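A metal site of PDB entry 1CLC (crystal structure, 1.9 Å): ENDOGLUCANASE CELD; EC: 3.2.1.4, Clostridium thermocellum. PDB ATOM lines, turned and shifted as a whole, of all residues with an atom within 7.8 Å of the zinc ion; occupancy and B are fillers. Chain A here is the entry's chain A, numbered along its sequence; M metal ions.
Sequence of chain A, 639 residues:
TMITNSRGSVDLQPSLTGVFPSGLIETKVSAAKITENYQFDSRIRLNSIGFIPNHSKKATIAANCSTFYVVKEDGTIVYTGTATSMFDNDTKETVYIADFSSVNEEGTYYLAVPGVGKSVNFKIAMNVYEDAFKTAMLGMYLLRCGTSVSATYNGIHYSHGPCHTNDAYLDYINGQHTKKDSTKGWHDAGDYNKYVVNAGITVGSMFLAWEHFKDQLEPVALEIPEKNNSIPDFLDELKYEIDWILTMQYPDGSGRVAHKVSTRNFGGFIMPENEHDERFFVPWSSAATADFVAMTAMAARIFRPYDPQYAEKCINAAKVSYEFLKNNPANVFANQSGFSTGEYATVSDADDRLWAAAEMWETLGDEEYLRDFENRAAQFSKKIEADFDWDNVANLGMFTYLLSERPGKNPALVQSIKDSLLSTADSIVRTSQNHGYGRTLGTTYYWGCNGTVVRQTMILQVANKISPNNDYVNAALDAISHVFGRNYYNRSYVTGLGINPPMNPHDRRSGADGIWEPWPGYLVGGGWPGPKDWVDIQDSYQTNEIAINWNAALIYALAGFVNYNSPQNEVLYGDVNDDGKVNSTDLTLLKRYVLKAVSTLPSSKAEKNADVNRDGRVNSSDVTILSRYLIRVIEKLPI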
ATOM      1  N   LEU A 143     -23.048 -20.188 -20.839  1.00  0.00           N
ATOM      2  CA  LEU A 143     -22.654 -21.580 -20.619  1.00  0.00           C
ATOM      3  C   LEU A 143     -23.671 -22.541 -21.266  1.00  0.00           C
ATOM      4  O   LEU A 143     -23.509 -23.749 -21.165  1.00  0.00           O
ATOM      5  CB  LEU A 143     -22.532 -21.908 -19.128  1.00  0.00           C
ATOM      6  CG  LEU A 143     -21.236 -21.545 -18.416  1.00  0.00           C
ATOM      7  CD1 LEU A 143     -21.386 -21.802 -16.939  1.00  0.00           C
ATOM      8  CD2 LEU A 143     -20.106 -22.351 -18.979  1.00  0.00           C
ATOM      9  N   ARG A 144     -24.697 -22.023 -21.925  1.00  0.00           N
ATOM     10  CA  ARG A 144     -25.709 -22.892 -22.501  1.00  0.00           C
ATOM     11  C   ARG A 144     -25.137 -23.835 -23.537  1.00  0.00           C
ATOM     12  O   ARG A 144     -24.318 -23.443 -24.377  1.00  0.00           O
ATOM     13  CB  ARG A 144     -26.853 -22.111 -23.110  1.00  0.00           C
ATOM     14  CG  ARG A 144     -27.832 -21.569 -22.106  1.00  0.00           C
ATOM     15  CD  ARG A 144     -28.927 -20.854 -22.840  1.00  0.00           C
ATOM     16  NE  ARG A 144     -29.767 -20.132 -21.904  1.00  0.00           N
ATOM     17  CZ  ARG A 144     -30.923 -19.573 -22.210  1.00  0.00           C
ATOM     18  NH1 ARG A 144     -31.410 -19.695 -23.448  1.00  0.00           N
ATOM     19  NH2 ARG A 144     -31.596 -18.909 -21.294  1.00  0.00           N
ATOM     20  N   CYS A 145     -25.702 -25.031 -23.556  1.00  0.00           N
ATOM     21  CA  CYS A 145     -25.271 -26.083 -24.459  1.00  0.00           C
ATOM     22  C   CYS A 145     -26.405 -26.412 -25.397  1.00  0.00           C
ATOM     23  O   CYS A 145     -27.563 -26.218 -25.048  1.00  0.00           O
ATOM     24  CB  CYS A 145     -24.917 -27.329 -23.635  1.00  0.00           C
ATOM     25  SG  CYS A 145     -24.231 -28.732 -24.569  1.00  0.00           S
ATOM     26  N   GLY A 146     -26.072 -26.888 -26.606  1.00  0.00           N
ATOM     27  CA  GLY A 146     -27.090 -27.280 -27.567  1.00  0.00           C
ATOM     28  C   GLY A 146     -27.702 -26.136 -28.329  1.00  0.00           C
ATOM     29  O   GLY A 146     -28.674 -26.323 -29.063  1.00  0.00           O
ATOM     30  N   THR A 147     -27.147 -24.944 -28.156  1.00  0.00           N
ATOM     31  CA  THR A 147     -27.668 -23.781 -28.839  1.00  0.00           C
ATOM     32  C   THR A 147     -26.560 -22.773 -29.082  1.00  0.00           C
ATOM     33  O   THR A 147     -25.492 -22.850 -28.478  1.00  0.00           O
ATOM     34  CB  THR A 147     -28.780 -23.097 -27.999  1.00  0.00           C
ATOM     35  OG1 THR A 147     -29.347 -22.030 -28.754  1.00  0.00           O
ATOM     36  CG2 THR A 147     -28.219 -22.505 -26.709  1.00  0.00           C
ATOM     37  N   HIS A 160     -20.889 -18.219 -29.916  1.00  0.00           N
ATOM     38  CA  HIS A 160     -20.461 -19.504 -30.433  1.00  0.00           C
ATOM     39  C   HIS A 160     -21.689 -20.149 -31.044  1.00  0.00           C
ATOM     40  O   HIS A 160     -22.816 -19.766 -30.715  1.00  0.00           O
ATOM     41  CB  HIS A 160     -19.762 -20.377 -29.378  1.00  0.00           C
ATOM     42  CG  HIS A 160     -20.667 -21.029 -28.377  1.00  0.00           C
ATOM     43  ND1 HIS A 160     -21.720 -21.833 -28.742  1.00  0.00           N
ATOM     44  CD2 HIS A 160     -20.613 -21.057 -27.026  1.00  0.00           C
ATOM     45  CE1 HIS A 160     -22.272 -22.353 -27.658  1.00  0.00           C
ATOM     46  NE2 HIS A 160     -21.618 -21.897 -26.600  1.00  0.00           N
ATOM     47  N   GLY A 161     -21.468 -20.999 -32.036  1.00  0.00           N
ATOM     48  CA  GLY A 161     -22.560 -21.667 -32.722  1.00  0.00           C
ATOM     49  C   GLY A 161     -23.104 -22.831 -31.944  1.00  0.00           C
ATOM     50  O   GLY A 161     -22.555 -23.190 -30.906  1.00  0.00           O
ATOM     51  N   PRO A 162     -24.187 -23.456 -32.441  1.00  0.00           N
ATOM     52  CA  PRO A 162     -24.854 -24.599 -31.827  1.00  0.00           C
ATOM     53  C   PRO A 162     -23.827 -25.659 -31.551  1.00  0.00           C
ATOM     54  O   PRO A 162     -23.009 -25.978 -32.408  1.00  0.00           O
ATOM     55  CB  PRO A 162     -25.816 -25.059 -32.902  1.00  0.00           C
ATOM     56  CG  PRO A 162     -26.108 -23.796 -33.654  1.00  0.00           C
ATOM     57  CD  PRO A 162     -24.754 -23.176 -33.771  1.00  0.00           C
ATOM     58  N   CYS A 163     -23.843 -26.195 -30.334  1.00  0.00           N
ATOM     59  CA  CYS A 163     -22.878 -27.197 -29.958  1.00  0.00           C
ATOM     60  C   CYS A 163     -23.589 -28.420 -29.391  1.00  0.00           C
ATOM     61  O   CYS A 163     -24.726 -28.336 -28.974  1.00  0.00           O
ATOM     62  CB  CYS A 163     -21.928 -26.611 -28.915  1.00  0.00           C
ATOM     63  SG  CYS A 163     -22.686 -26.208 -27.304  1.00  0.00           S
ATOM     64  N   HIS A 164     -22.893 -29.557 -29.403  1.00  0.00           N
ATOM     65  CA  HIS A 164     -23.412 -30.821 -28.879  1.00  0.00           C
ATOM     66  C   HIS A 164     -24.867 -31.104 -29.177  1.00  0.00           C
ATOM     67  O   HIS A 164     -25.655 -31.477 -28.304  1.00  0.00           O
ATOM     68  CB  HIS A 164     -23.090 -30.889 -27.394  1.00  0.00           C
ATOM     69  CG  HIS A 164     -21.648 -30.578 -27.094  1.00  0.00           C
ATOM     70  ND1 HIS A 164     -21.201 -29.297 -26.858  1.00  0.00           N
ATOM     71  CD2 HIS A 164     -20.550 -31.370 -27.044  1.00  0.00           C
ATOM     72  CE1 HIS A 164     -19.894 -29.313 -26.653  1.00  0.00           C
ATOM     73  NE2 HIS A 164     -19.484 -30.550 -26.767  1.00  0.00           N
ATOM     74  N   THR A 165     -25.172 -30.976 -30.510  1.00  0.00           N
ATOM     75  CA  THR A 165     -26.557 -31.175 -30.900  1.00  0.00           C
ATOM     76  C   THR A 165     -26.914 -32.638 -31.074  1.00  0.00           C
ATOM     77  O   THR A 165     -28.070 -32.965 -31.314  1.00  0.00           O
ATOM     78  CB  THR A 165     -26.887 -30.370 -32.146  1.00  0.00           C
ATOM     79  OG1 THR A 165     -26.002 -30.753 -33.197  1.00  0.00           O
ATOM     80  CG2 THR A 165     -26.761 -28.881 -31.859  1.00  0.00           C
ATOM     81  N   ASP A 167     -26.312 -35.058 -28.590  1.00  0.00           N
ATOM     82  CA  ASP A 167     -26.309 -35.728 -27.287  1.00  0.00           C
ATOM     83  C   ASP A 167     -27.614 -36.551 -27.332  1.00  0.00           C
ATOM     84  O   ASP A 167     -28.661 -36.012 -27.688  1.00  0.00           O
ATOM     85  CB  ASP A 167     -26.498 -34.730 -26.112  1.00  0.00           C
ATOM     86  CG  ASP A 167     -25.358 -33.770 -25.958  1.00  0.00           C
ATOM     87  OD1 ASP A 167     -24.354 -33.937 -26.666  1.00  0.00           O
ATOM     88  OD2 ASP A 167     -25.418 -32.906 -25.069  1.00  0.00           O
ATOM     89  N   LYS A 184     -29.408 -29.314 -24.656  1.00  0.00           N
ATOM     90  CA  LYS A 184     -29.701 -28.229 -23.733  1.00  0.00           C
ATOM     91  C   LYS A 184     -28.906 -28.341 -22.450  1.00  0.00           C
ATOM     92  O   LYS A 184     -27.986 -29.141 -22.353  1.00  0.00           O
ATOM     93  CB  LYS A 184     -31.189 -28.137 -23.445  1.00  0.00           C
ATOM     94  CG  LYS A 184     -31.990 -27.807 -24.690  1.00  0.00           C
ATOM     95  CD  LYS A 184     -33.379 -27.417 -24.280  1.00  0.00           C
ATOM     96  CE  LYS A 184     -34.155 -26.882 -25.448  1.00  0.00           C
ATOM     97  NZ  LYS A 184     -35.370 -26.145 -24.972  1.00  0.00           N
ATOM     98  N   GLY A 185     -29.248 -27.504 -21.470  1.00  0.00           N
ATOM     99  CA  GLY A 185     -28.527 -27.499 -20.215  1.00  0.00           C
ATOM    100  C   GLY A 185     -27.305 -26.592 -20.312  1.00  0.00           C
ATOM    101  O   GLY A 185     -27.078 -25.921 -21.315  1.00  0.00           O
ATOM    102  N   TRP A 186     -26.510 -26.587 -19.259  1.00  0.00           N
ATOM    103  CA  TRP A 186     -25.324 -25.765 -19.234  1.00  0.00           C
ATOM    104  C   TRP A 186     -24.077 -26.637 -19.214  1.00  0.00           C
ATOM    105  O   TRP A 186     -24.059 -27.696 -18.545  1.00  0.00           O
ATOM    106  CB  TRP A 186     -25.263 -24.940 -17.933  1.00  0.00           C
ATOM    107  CG  TRP A 186     -26.402 -23.990 -17.649  1.00  0.00           C
ATOM    108  CD1 TRP A 186     -26.919 -23.038 -18.475  1.00  0.00           C
ATOM    109  CD2 TRP A 186     -27.132 -23.899 -16.435  1.00  0.00           C
ATOM    110  NE1 TRP A 186     -27.942 -22.363 -17.846  1.00  0.00           N
ATOM    111  CE2 TRP A 186     -28.086 -22.881 -16.584  1.00  0.00           C
ATOM    112  CE3 TRP A 186     -27.072 -24.599 -15.218  1.00  0.00           C
ATOM    113  CZ2 TRP A 186     -28.979 -22.533 -15.573  1.00  0.00           C
ATOM    114  CZ3 TRP A 186     -27.961 -24.260 -14.218  1.00  0.00           C
ATOM    115  CH2 TRP A 186     -28.906 -23.235 -14.405  1.00  0.00           C
ATOM    116  N   HIS A 187     -23.018 -26.171 -19.885  1.00  0.00           N
ATOM    117  CA  HIS A 187     -21.728 -26.831 -19.814  1.00  0.00           C
ATOM    118  C   HIS A 187     -21.374 -26.675 -18.363  1.00  0.00           C
ATOM    119  O   HIS A 187     -21.606 -25.612 -17.775  1.00  0.00           O
ATOM    120  CB  HIS A 187     -20.699 -26.073 -20.617  1.00  0.00           C
ATOM    121  CG  HIS A 187     -20.970 -26.084 -22.072  1.00  0.00           C
ATOM    122  ND1 HIS A 187     -21.001 -24.941 -22.833  1.00  0.00           N
ATOM    123  CD2 HIS A 187     -21.198 -27.111 -22.929  1.00  0.00           C
ATOM    124  CE1 HIS A 187     -21.219 -25.253 -24.089  1.00  0.00           C
ATOM    125  NE2 HIS A 187     -21.339 -26.557 -24.183  1.00  0.00           N
ATOM    126  N   TYR A 192     -17.009 -29.068 -21.363  1.00  0.00           N
ATOM    127  CA  TYR A 192     -18.367 -29.018 -21.889  1.00  0.00           C
ATOM    128  C   TYR A 192     -19.355 -30.117 -21.485  1.00  0.00           C
ATOM    129  O   TYR A 192     -20.488 -30.101 -21.949  1.00  0.00           O
ATOM    130  CB  TYR A 192     -18.332 -28.982 -23.414  1.00  0.00           C
ATOM    131  CG  TYR A 192     -17.510 -27.858 -23.982  1.00  0.00           C
ATOM    132  CD1 TYR A 192     -17.686 -26.544 -23.521  1.00  0.00           C
ATOM    133  CD2 TYR A 192     -16.557 -28.098 -24.979  1.00  0.00           C
ATOM    134  CE1 TYR A 192     -16.953 -25.498 -24.042  1.00  0.00           C
ATOM    135  CE2 TYR A 192     -15.809 -27.048 -25.516  1.00  0.00           C
ATOM    136  CZ  TYR A 192     -16.010 -25.761 -25.035  1.00  0.00           C
ATOM    137  OH  TYR A 192     -15.297 -24.707 -25.560  1.00  0.00           O
ATOM    138  N   ASN A 193     -18.925 -31.051 -20.646  1.00  0.00           N
ATOM    139  CA  ASN A 193     -19.792 -32.147 -20.232  1.00  0.00           C
ATOM    140  C   ASN A 193     -20.838 -31.696 -19.220  1.00  0.00           C
ATOM    141  O   ASN A 193     -20.657 -30.673 -18.575  1.00  0.00           O
ATOM    142  CB  ASN A 193     -18.935 -33.294 -19.722  1.00  0.00           C
ATOM    143  CG  ASN A 193     -17.897 -33.713 -20.751  1.00  0.00           C
ATOM    144  OD1 ASN A 193     -18.242 -34.071 -21.870  1.00  0.00           O
ATOM    145  ND2 ASN A 193     -16.628 -33.528 -20.425  1.00  0.00           N
ATOM    146  N   LYS A 194     -21.952 -32.412 -19.154  1.00  0.00           N
ATOM    147  CA  LYS A 194     -23.060 -32.060 -18.271  1.00  0.00           C
ATOM    148  C   LYS A 194     -23.227 -33.129 -17.222  1.00  0.00           C
ATOM    149  O   LYS A 194     -23.408 -34.291 -17.557  1.00  0.00           O
ATOM    150  CB  LYS A 194     -24.311 -31.866 -19.120  1.00  0.00           C
ATOM    151  CG  LYS A 194     -24.045 -30.970 -20.292  1.00  0.00           C
ATOM    152  CD  LYS A 194     -25.250 -30.631 -21.123  1.00  0.00           C
ATOM    153  CE  LYS A 194     -25.761 -31.812 -21.924  1.00  0.00           C
ATOM    154  NZ  LYS A 194     -26.606 -31.359 -23.083  1.00  0.00           N
ATOM    155  N   PRO A 272     -16.912 -25.026 -28.453  1.00  0.00           N
ATOM    156  CA  PRO A 272     -17.847 -26.149 -28.313  1.00  0.00           C
ATOM    157  C   PRO A 272     -18.490 -26.693 -29.584  1.00  0.00           C
ATOM    158  O   PRO A 272     -18.680 -27.898 -29.719  1.00  0.00           O
ATOM    159  CB  PRO A 272     -18.851 -25.624 -27.287  1.00  0.00           C
ATOM    160  CG  PRO A 272     -18.917 -24.159 -27.588  1.00  0.00           C
ATOM    161  CD  PRO A 272     -17.459 -23.804 -27.821  1.00  0.00           C
ATOM    162  N   GLU A 273     -18.774 -25.824 -30.555  1.00  0.00           N
ATOM    163  CA  GLU A 273     -19.381 -26.287 -31.791  1.00  0.00           C
ATOM    164  C   GLU A 273     -18.412 -27.099 -32.638  1.00  0.00           C
ATOM    165  O   GLU A 273     -18.801 -27.662 -33.649  1.00  0.00           O
ATOM    166  CB  GLU A 273     -19.948 -25.118 -32.611  1.00  0.00           C
ATOM    167  CG  GLU A 273     -18.912 -24.155 -33.153  1.00  0.00           C
ATOM    168  CD  GLU A 273     -18.685 -22.939 -32.273  1.00  0.00           C
ATOM    169  OE1 GLU A 273     -18.438 -23.117 -31.058  1.00  0.00           O
ATOM    170  OE2 GLU A 273     -18.744 -21.803 -32.811  1.00  0.00           O
ATOM    171  N   GLU A 275     -16.562 -29.465 -31.178  1.00  0.00           N
ATOM    172  CA  GLU A 275     -16.357 -30.743 -30.524  1.00  0.00           C
ATOM    173  C   GLU A 275     -17.339 -31.714 -31.143  1.00  0.00           C
ATOM    174  O   GLU A 275     -18.554 -31.638 -30.936  1.00  0.00           O
ATOM    175  CB  GLU A 275     -16.531 -30.672 -29.014  1.00  0.00           C
ATOM    176  CG  GLU A 275     -16.079 -31.931 -28.356  1.00  0.00           C
ATOM    177  CD  GLU A 275     -16.022 -31.829 -26.865  1.00  0.00           C
ATOM    178  OE1 GLU A 275     -17.046 -31.455 -26.260  1.00  0.00           O
ATOM    179  OE2 GLU A 275     -14.967 -32.157 -26.290  1.00  0.00           O
ATOM    180  N   ARG A 279     -21.080 -38.137 -27.521  1.00  0.00           N
ATOM    181  CA  ARG A 279     -21.304 -37.979 -26.081  1.00  0.00           C
ATOM    182  C   ARG A 279     -22.294 -39.058 -25.674  1.00  0.00           C
ATOM    183  O   ARG A 279     -23.250 -39.337 -26.399  1.00  0.00           O
ATOM    184  CB  ARG A 279     -21.818 -36.569 -25.783  1.00  0.00           C
ATOM    185  CG  ARG A 279     -20.916 -35.494 -26.361  1.00  0.00           C
ATOM    186  CD  ARG A 279     -20.617 -34.420 -25.361  1.00  0.00           C
ATOM    187  NE  ARG A 279     -21.774 -33.576 -25.133  1.00  0.00           N
ATOM    188  CZ  ARG A 279     -21.794 -32.559 -24.279  1.00  0.00           C
ATOM    189  NH1 ARG A 279     -20.697 -32.242 -23.626  1.00  0.00           N
ATOM    190  NH2 ARG A 279     -22.891 -31.839 -24.121  1.00  0.00           N
HETATM  191 ZN    ZN M   1     -22.464 -27.761 -25.784  1.00  0.00          ZN
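A ring nitrogen (NE2) of His 164 sits at hydrogen-bond distance from the side-chain carboxylate (OE1) of Glu 275, at 2.6 Å. The side-chain sulfur (SG) of Cys 145 sits close to the guanidinium group (NH2) of Arg 279, at 3.4 Å. O of Leu 143 sits at hydrogen-bond distance from N of His 187, at 2.8 Å. The backbone NH (N) of Cys 145 sits at hydrogen-bond distance from the backbone carbonyl oxygen (O) of Gly 185 (2.8 Å). The backbone NH (N) of Gly 146 lies close to the backbone carbonyl oxygen (O) of Cys 163, 3.1 Å away.
Residues that only touch the zinc ion: Gly 146 (3.8 Å). Within 4 Å of the zinc ion: Cys 145, Gly 146, Cys 163, His 164 and His 187. The nearest printed residue that does not touch the zinc ion is Arg 279 (4.4 Å).
The zinc ion is bound by the side-chain sulfur (SG) of Cys 163 (2.2 Å), a ring nitrogen (ND1) of His 164 (2.3 Å), a ring nitrogen (NE2) of His 187 (2.3 Å) and the side-chain sulfur (SG) of Cys 145 (2.4 Å). The zinc ion has four donor atoms within binding distance.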
